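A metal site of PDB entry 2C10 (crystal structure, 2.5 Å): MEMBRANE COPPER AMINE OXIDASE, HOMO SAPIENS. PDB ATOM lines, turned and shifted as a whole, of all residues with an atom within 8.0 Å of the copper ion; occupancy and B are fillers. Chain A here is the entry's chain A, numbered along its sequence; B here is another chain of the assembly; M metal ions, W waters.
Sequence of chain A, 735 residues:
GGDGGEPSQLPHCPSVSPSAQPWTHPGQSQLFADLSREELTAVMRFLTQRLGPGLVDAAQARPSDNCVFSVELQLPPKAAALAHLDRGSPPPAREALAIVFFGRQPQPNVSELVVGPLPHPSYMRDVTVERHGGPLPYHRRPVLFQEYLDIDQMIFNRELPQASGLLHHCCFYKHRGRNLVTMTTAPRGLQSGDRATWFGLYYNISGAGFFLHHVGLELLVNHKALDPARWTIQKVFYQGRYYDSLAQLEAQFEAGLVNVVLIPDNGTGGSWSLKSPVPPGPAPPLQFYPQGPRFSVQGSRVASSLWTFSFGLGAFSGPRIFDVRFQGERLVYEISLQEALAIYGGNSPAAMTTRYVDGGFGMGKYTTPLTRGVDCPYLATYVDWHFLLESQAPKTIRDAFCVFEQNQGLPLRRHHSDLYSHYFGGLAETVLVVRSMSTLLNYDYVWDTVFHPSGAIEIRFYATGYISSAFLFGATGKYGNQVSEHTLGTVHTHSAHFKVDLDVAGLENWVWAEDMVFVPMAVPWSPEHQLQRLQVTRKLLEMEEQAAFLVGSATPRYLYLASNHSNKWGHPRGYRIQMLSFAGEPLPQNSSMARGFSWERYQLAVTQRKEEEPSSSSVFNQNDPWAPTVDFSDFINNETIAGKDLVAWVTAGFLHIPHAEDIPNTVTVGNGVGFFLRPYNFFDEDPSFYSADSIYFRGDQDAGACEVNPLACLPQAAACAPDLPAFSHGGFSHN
N of His 494 sits at hydrogen-bond distance from O of Phe 654, 2.9 Å away.
NE2 of His 656 is in hydrogen-bond range of OD2 of Asp 662 (2.7 Å).
A ring nitrogen (ND1) of His 492 is in hydrogen-bond range of the backbone carbonyl oxygen (O) of Thr 490 (2.8 Å).
The nearest printed residue that does not touch the copper ion is TPQ 443 (4.3 Å).
The copper ion is bound by NE2 of His 494 (2.0 Å), ND1 of His 656 (2.0 Å), NE2 of His 492 (2.2 Å) and water W1 (2.4 Å).
The copper ion has four donor atoms within binding distance.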
ATOM      1  N   ALA A 342      22.509  20.193   8.390  1.00  0.00           N
ATOM      2  CA  ALA A 342      21.440  19.467   9.086  1.00  0.00           C
ATOM      3  C   ALA A 342      20.157  19.744   8.342  1.00  0.00           C
ATOM      4  O   ALA A 342      19.759  20.905   8.214  1.00  0.00           O
ATOM      5  CB  ALA A 342      21.335  19.893  10.524  1.00  0.00           C
ATOM      6  N   TYR A 344      16.156  19.057   8.133  1.00  0.00           N
ATOM      7  CA  TYR A 344      15.083  18.720   9.076  1.00  0.00           C
ATOM      8  C   TYR A 344      13.752  18.320   8.408  1.00  0.00           C
ATOM      9  O   TYR A 344      13.456  18.692   7.268  1.00  0.00           O
ATOM     10  CB  TYR A 344      14.856  19.894  10.050  1.00  0.00           C
ATOM     11  CG  TYR A 344      15.801  19.861  11.236  1.00  0.00           C
ATOM     12  CD1 TYR A 344      15.436  19.205  12.404  1.00  0.00           C
ATOM     13  CD2 TYR A 344      17.053  20.462  11.175  1.00  0.00           C
ATOM     14  CE1 TYR A 344      16.304  19.142  13.502  1.00  0.00           C
ATOM     15  CE2 TYR A 344      17.931  20.426  12.274  1.00  0.00           C
ATOM     16  CZ  TYR A 344      17.551  19.753  13.432  1.00  0.00           C
ATOM     17  OH  TYR A 344      18.391  19.677  14.532  1.00  0.00           O
ATOM     18  N   ASN A 442      21.509  24.359  19.390  1.00  0.00           N
ATOM     19  CA  ASN A 442      21.275  23.178  20.248  1.00  0.00           C
ATOM     20  C   ASN A 442      22.398  22.152  20.228  1.00  0.00           C
ATOM     21  O   ASN A 442      22.589  21.444  21.210  1.00  0.00           O
ATOM     22  CB  ASN A 442      19.959  22.488  19.897  1.00  0.00           C
ATOM     23  CG  ASN A 442      19.825  22.241  18.421  1.00  0.00           C
ATOM     24  OD1 ASN A 442      19.703  23.175  17.645  1.00  0.00           O
ATOM     25  ND2 ASN A 442      19.855  20.970  18.016  1.00  0.00           N
ATOM     26  N   TPQ A 443      23.121  22.041  19.128  1.00  0.00           N
ATOM     27  CA  TPQ A 443      24.049  20.931  19.026  1.00  0.00           C
ATOM     28  CB  TPQ A 443      23.825  19.995  17.828  1.00  0.00           C
ATOM     29  C   TPQ A 443      25.497  21.273  19.224  1.00  0.00           C
ATOM     30  O   TPQ A 443      25.932  22.442  19.076  1.00  0.00           O
ATOM     31  C1  TPQ A 443      23.477  20.631  16.512  1.00  0.00           C
ATOM     32  C2  TPQ A 443      22.358  20.027  15.732  1.00  0.00           C
ATOM     33  O2  TPQ A 443      21.690  18.967  16.270  1.00  0.00           O
ATOM     34  C3  TPQ A 443      21.970  20.519  14.492  1.00  0.00           C
ATOM     35  C4  TPQ A 443      22.680  21.608  13.973  1.00  0.00           C
ATOM     36  O4  TPQ A 443      22.361  22.141  12.750  1.00  0.00           O
ATOM     37  C5  TPQ A 443      23.811  22.208  14.732  1.00  0.00           C
ATOM     38  O5  TPQ A 443      24.445  23.266  14.155  1.00  0.00           O
ATOM     39  C6  TPQ A 443      24.195  21.703  15.981  1.00  0.00           C
ATOM     40  N   TYR A 445      29.031  19.877  17.912  1.00  0.00           N
ATOM     41  CA  TYR A 445      29.902  19.111  17.066  1.00  0.00           C
ATOM     42  C   TYR A 445      31.282  18.927  17.738  1.00  0.00           C
ATOM     43  O   TYR A 445      31.907  19.902  18.162  1.00  0.00           O
ATOM     44  CB  TYR A 445      30.100  19.855  15.751  1.00  0.00           C
ATOM     45  CG  TYR A 445      28.862  19.997  14.869  1.00  0.00           C
ATOM     46  CD1 TYR A 445      28.365  21.258  14.540  1.00  0.00           C
ATOM     47  CD2 TYR A 445      28.256  18.875  14.318  1.00  0.00           C
ATOM     48  CE1 TYR A 445      27.237  21.405  13.691  1.00  0.00           C
ATOM     49  CE2 TYR A 445      27.137  19.003  13.488  1.00  0.00           C
ATOM     50  CZ  TYR A 445      26.642  20.263  13.178  1.00  0.00           C
ATOM     51  OH  TYR A 445      25.545  20.367  12.346  1.00  0.00           O
ATOM     52  N   ALA A 463      28.024  14.396  16.815  1.00  0.00           N
ATOM     53  CA  ALA A 463      27.025  15.417  17.107  1.00  0.00           C
ATOM     54  C   ALA A 463      26.358  15.043  18.415  1.00  0.00           C
ATOM     55  O   ALA A 463      25.677  14.019  18.494  1.00  0.00           O
ATOM     56  CB  ALA A 463      26.009  15.512  15.989  1.00  0.00           C
ATOM     57  N   THR A 464      26.594  15.864  19.437  1.00  0.00           N
ATOM     58  CA  THR A 464      26.015  15.661  20.767  1.00  0.00           C
ATOM     59  C   THR A 464      25.273  16.962  21.096  1.00  0.00           C
ATOM     60  O   THR A 464      24.971  17.725  20.173  1.00  0.00           O
ATOM     61  CB  THR A 464      27.103  15.261  21.829  1.00  0.00           C
ATOM     62  OG1 THR A 464      26.535  15.175  23.142  1.00  0.00           O
ATOM     63  CG2 THR A 464      28.263  16.234  21.829  1.00  0.00           C
ATOM     64  N   GLY A 465      25.000  17.212  22.376  1.00  0.00           N
ATOM     65  CA  GLY A 465      24.200  18.383  22.773  1.00  0.00           C
ATOM     66  C   GLY A 465      22.703  18.138  22.762  1.00  0.00           C
ATOM     67  O   GLY A 465      22.252  16.999  22.843  1.00  0.00           O
ATOM     68  N   TYR A 466      21.922  19.198  22.652  1.00  0.00           N
ATOM     69  CA  TYR A 466      20.477  19.077  22.614  1.00  0.00           C
ATOM     70  C   TYR A 466      19.970  18.809  21.199  1.00  0.00           C
ATOM     71  O   TYR A 466      20.538  19.281  20.212  1.00  0.00           O
ATOM     72  CB  TYR A 466      19.828  20.363  23.147  1.00  0.00           C
ATOM     73  CG  TYR A 466      19.838  20.452  24.654  1.00  0.00           C
ATOM     74  CD1 TYR A 466      20.855  21.126  25.332  1.00  0.00           C
ATOM     75  CD2 TYR A 466      18.838  19.842  25.400  1.00  0.00           C
ATOM     76  CE1 TYR A 466      20.862  21.187  26.738  1.00  0.00           C
ATOM     77  CE2 TYR A 466      18.827  19.896  26.797  1.00  0.00           C
ATOM     78  CZ  TYR A 466      19.839  20.557  27.465  1.00  0.00           C
ATOM     79  OH  TYR A 466      19.799  20.598  28.843  1.00  0.00           O
ATOM     80  N   ILE A 467      18.887  18.043  21.102  1.00  0.00           N
ATOM     81  CA  ILE A 467      18.107  18.023  19.875  1.00  0.00           C
ATOM     82  C   ILE A 467      17.264  19.288  19.737  1.00  0.00           C
ATOM     83  O   ILE A 467      16.955  19.994  20.707  1.00  0.00           O
ATOM     84  CB  ILE A 467      17.197  16.763  19.768  1.00  0.00           C
ATOM     85  CG1 ILE A 467      16.116  16.766  20.845  1.00  0.00           C
ATOM     86  CG2 ILE A 467      18.020  15.462  19.805  1.00  0.00           C
ATOM     87  CD1 ILE A 467      15.038  15.827  20.561  1.00  0.00           C
ATOM     88  N   SER A 468      16.888  19.586  18.498  1.00  0.00           N
ATOM     89  CA  SER A 468      15.937  20.637  18.188  1.00  0.00           C
ATOM     90  C   SER A 468      14.545  20.011  18.306  1.00  0.00           C
ATOM     91  O   SER A 468      14.339  18.890  17.851  1.00  0.00           O
ATOM     92  CB  SER A 468      16.173  21.097  16.758  1.00  0.00           C
ATOM     93  OG  SER A 468      15.827  22.457  16.635  1.00  0.00           O
ATOM     94  N   THR A 490      12.294  16.191  16.349  1.00  0.00           N
ATOM     95  CA  THR A 490      12.158  16.307  14.868  1.00  0.00           C
ATOM     96  C   THR A 490      13.238  15.568  14.070  1.00  0.00           C
ATOM     97  O   THR A 490      14.445  15.743  14.286  1.00  0.00           O
ATOM     98  CB  THR A 490      12.189  17.774  14.415  1.00  0.00           C
ATOM     99  OG1 THR A 490      13.390  18.391  14.909  1.00  0.00           O
ATOM    100  CG2 THR A 490      10.969  18.525  14.910  1.00  0.00           C
ATOM    101  N   VAL A 491      12.796  14.769  13.112  1.00  0.00           N
ATOM    102  CA  VAL A 491      13.694  13.947  12.302  1.00  0.00           C
ATOM    103  C   VAL A 491      14.632  14.829  11.500  1.00  0.00           C
ATOM    104  O   VAL A 491      14.255  15.919  11.096  1.00  0.00           O
ATOM    105  CB  VAL A 491      12.910  12.965  11.406  1.00  0.00           C
ATOM    106  CG1 VAL A 491      11.942  13.687  10.462  1.00  0.00           C
ATOM    107  CG2 VAL A 491      13.844  12.045  10.651  1.00  0.00           C
ATOM    108  N   HIS A 492      15.861  14.371  11.307  1.00  0.00           N
ATOM    109  CA  HIS A 492      16.847  15.151  10.548  1.00  0.00           C
ATOM    110  C   HIS A 492      18.081  14.338  10.250  1.00  0.00           C
ATOM    111  O   HIS A 492      18.358  13.348  10.945  1.00  0.00           O
ATOM    112  CB  HIS A 492      17.288  16.368  11.354  1.00  0.00           C
ATOM    113  CG  HIS A 492      17.931  16.023  12.655  1.00  0.00           C
ATOM    114  ND1 HIS A 492      17.201  15.721  13.779  1.00  0.00           N
ATOM    115  CD2 HIS A 492      19.238  15.872  12.991  1.00  0.00           C
ATOM    116  CE1 HIS A 492      18.028  15.426  14.770  1.00  0.00           C
ATOM    117  NE2 HIS A 492      19.263  15.506  14.318  1.00  0.00           N
ATOM    118  N   THR A 493      18.831  14.796   9.241  1.00  0.00           N
ATOM    119  CA  THR A 493      20.119  14.198   8.899  1.00  0.00           C
ATOM    120  C   THR A 493      21.255  15.135   9.270  1.00  0.00           C
ATOM    121  O   THR A 493      21.086  16.360   9.251  1.00  0.00           O
ATOM    122  CB  THR A 493      20.237  13.904   7.386  1.00  0.00           C
ATOM    123  OG1 THR A 493      20.063  15.121   6.654  1.00  0.00           O
ATOM    124  CG2 THR A 493      19.196  12.895   6.936  1.00  0.00           C
ATOM    125  N   HIS A 494      22.415  14.564   9.608  1.00  0.00           N
ATOM    126  CA  HIS A 494      23.651  15.311   9.735  1.00  0.00           C
ATOM    127  C   HIS A 494      24.621  14.928   8.629  1.00  0.00           C
ATOM    128  O   HIS A 494      24.719  13.775   8.245  1.00  0.00           O
ATOM    129  CB  HIS A 494      24.316  15.017  11.067  1.00  0.00           C
ATOM    130  CG  HIS A 494      23.490  15.383  12.265  1.00  0.00           C
ATOM    131  ND1 HIS A 494      23.533  16.631  12.845  1.00  0.00           N
ATOM    132  CD2 HIS A 494      22.654  14.637  13.036  1.00  0.00           C
ATOM    133  CE1 HIS A 494      22.742  16.647  13.905  1.00  0.00           C
ATOM    134  NE2 HIS A 494      22.208  15.454  14.049  1.00  0.00           N
ATOM    135  N   PHE A 654      24.697  10.824   8.857  1.00  0.00           N
ATOM    136  CA  PHE A 654      23.741   9.804   9.283  1.00  0.00           C
ATOM    137  C   PHE A 654      22.362  10.417   9.441  1.00  0.00           C
ATOM    138  O   PHE A 654      22.221  11.636   9.530  1.00  0.00           O
ATOM    139  CB  PHE A 654      24.187   9.147  10.593  1.00  0.00           C
ATOM    140  CG  PHE A 654      24.459  10.134  11.690  1.00  0.00           C
ATOM    141  CD1 PHE A 654      23.468  10.476  12.616  1.00  0.00           C
ATOM    142  CD2 PHE A 654      25.718  10.737  11.810  1.00  0.00           C
ATOM    143  CE1 PHE A 654      23.721  11.404  13.631  1.00  0.00           C
ATOM    144  CE2 PHE A 654      25.989  11.673  12.835  1.00  0.00           C
ATOM    145  CZ  PHE A 654      24.974  11.994  13.741  1.00  0.00           C
ATOM    146  N   LEU A 655      21.333   9.568   9.458  1.00  0.00           N
ATOM    147  CA  LEU A 655      19.992   9.991   9.746  1.00  0.00           C
ATOM    148  C   LEU A 655      19.831   9.924  11.247  1.00  0.00           C
ATOM    149  O   LEU A 655      20.302   8.984  11.882  1.00  0.00           O
ATOM    150  CB  LEU A 655      19.000   9.051   9.096  1.00  0.00           C
ATOM    151  CG  LEU A 655      17.536   9.109   9.547  1.00  0.00           C
ATOM    152  CD1 LEU A 655      16.874  10.374   9.007  1.00  0.00           C
ATOM    153  CD2 LEU A 655      16.813   7.863   9.048  1.00  0.00           C
ATOM    154  N   HIS A 656      19.165  10.914  11.809  1.00  0.00           N
ATOM    155  CA  HIS A 656      18.898  10.926  13.229  1.00  0.00           C
ATOM    156  C   HIS A 656      17.386  11.073  13.497  1.00  0.00           C
ATOM    157  O   HIS A 656      16.804  12.145  13.265  1.00  0.00           O
ATOM    158  CB  HIS A 656      19.753  11.999  13.914  1.00  0.00           C
ATOM    159  CG  HIS A 656      19.600  12.058  15.399  1.00  0.00           C
ATOM    160  ND1 HIS A 656      20.072  13.106  16.146  1.00  0.00           N
ATOM    161  CD2 HIS A 656      18.981  11.207  16.264  1.00  0.00           C
ATOM    162  CE1 HIS A 656      19.767  12.900  17.419  1.00  0.00           C
ATOM    163  NE2 HIS A 656      19.110  11.754  17.512  1.00  0.00           N
ATOM    164  N   ILE A 657      16.751   9.980  13.931  1.00  0.00           N
ATOM    165  CA  ILE A 657      15.347  10.002  14.337  1.00  0.00           C
ATOM    166  C   ILE A 657      15.348  10.063  15.863  1.00  0.00           C
ATOM    167  O   ILE A 657      15.587   9.057  16.530  1.00  0.00           O
ATOM    168  CB  ILE A 657      14.576   8.742  13.870  1.00  0.00           C
ATOM    169  CG1 ILE A 657      14.934   8.411  12.421  1.00  0.00           C
ATOM    170  CG2 ILE A 657      13.087   8.951  14.048  1.00  0.00           C
ATOM    171  CD1 ILE A 657      14.266   7.183  11.870  1.00  0.00           C
ATOM    172  N   PRO A 658      15.141  11.253  16.416  1.00  0.00           N
ATOM    173  CA  PRO A 658      15.243  11.376  17.869  1.00  0.00           C
ATOM    174  C   PRO A 658      14.373  10.364  18.601  1.00  0.00           C
ATOM    175  O   PRO A 658      13.329   9.931  18.095  1.00  0.00           O
ATOM    176  CB  PRO A 658      14.752  12.797  18.137  1.00  0.00           C
ATOM    177  CG  PRO A 658      15.077  13.530  16.864  1.00  0.00           C
ATOM    178  CD  PRO A 658      14.805  12.543  15.777  1.00  0.00           C
ATOM    179  N   ASP A 662      17.694  10.473  23.650  1.00  0.00           N
ATOM    180  CA  ASP A 662      18.334  11.751  23.283  1.00  0.00           C
ATOM    181  C   ASP A 662      18.027  12.841  24.319  1.00  0.00           C
ATOM    182  O   ASP A 662      18.415  13.990  24.133  1.00  0.00           O
ATOM    183  CB  ASP A 662      17.869  12.229  21.897  1.00  0.00           C
ATOM    184  CG  ASP A 662      18.504  11.443  20.724  1.00  0.00           C
ATOM    185  OD1 ASP A 662      19.711  11.123  20.769  1.00  0.00           O
ATOM    186  OD2 ASP A 662      17.776  11.165  19.733  1.00  0.00           O
ATOM    187  N   THR A 666      21.875  14.094  23.127  1.00  0.00           N
ATOM    188  CA  THR A 666      22.234  12.998  22.228  1.00  0.00           C
ATOM    189  C   THR A 666      23.643  12.537  22.616  1.00  0.00           C
ATOM    190  O   THR A 666      24.566  13.356  22.645  1.00  0.00           O
ATOM    191  CB  THR A 666      22.270  13.458  20.741  1.00  0.00           C
ATOM    192  OG1 THR A 666      21.012  14.050  20.400  1.00  0.00           O
ATOM    193  CG2 THR A 666      22.507  12.287  19.796  1.00  0.00           C
ATOM    194  N   ASN A 671      27.835   7.108  17.168  1.00  0.00           N
ATOM    195  CA  ASN A 671      27.360   8.233  16.381  1.00  0.00           C
ATOM    196  C   ASN A 671      28.502   9.103  15.857  1.00  0.00           C
ATOM    197  O   ASN A 671      28.320  10.312  15.647  1.00  0.00           O
ATOM    198  CB  ASN A 671      26.434   9.095  17.234  1.00  0.00           C
ATOM    199  CG  ASN A 671      25.000   8.616  17.190  1.00  0.00           C
ATOM    200  OD1 ASN A 671      24.581   7.914  16.254  1.00  0.00           O
ATOM    201  ND2 ASN A 671      24.223   9.028  18.196  1.00  0.00           N
ATOM    202  N   TYR B 558      17.417   2.419  10.312  1.00  0.00           N
ATOM    203  CA  TYR B 558      17.078   2.037  11.690  1.00  0.00           C
ATOM    204  C   TYR B 558      16.405   0.679  11.705  1.00  0.00           C
ATOM    205  O   TYR B 558      15.244   0.557  11.338  1.00  0.00           O
ATOM    206  CB  TYR B 558      16.141   3.049  12.349  1.00  0.00           C
ATOM    207  CG  TYR B 558      16.813   4.291  12.891  1.00  0.00           C
ATOM    208  CD1 TYR B 558      17.296   5.267  12.020  1.00  0.00           C
ATOM    209  CD2 TYR B 558      16.948   4.502  14.256  1.00  0.00           C
ATOM    210  CE1 TYR B 558      17.904   6.428  12.503  1.00  0.00           C
ATOM    211  CE2 TYR B 558      17.551   5.650  14.738  1.00  0.00           C
ATOM    212  CZ  TYR B 558      18.024   6.623  13.847  1.00  0.00           C
ATOM    213  OH  TYR B 558      18.633   7.776  14.289  1.00  0.00           O
HETATM  214 CU    CU M   1      20.961  14.825  15.522  1.00  0.00          CU
HETATM  215  O   HOH W   1      20.776  16.628  17.081  1.00  0.00           O
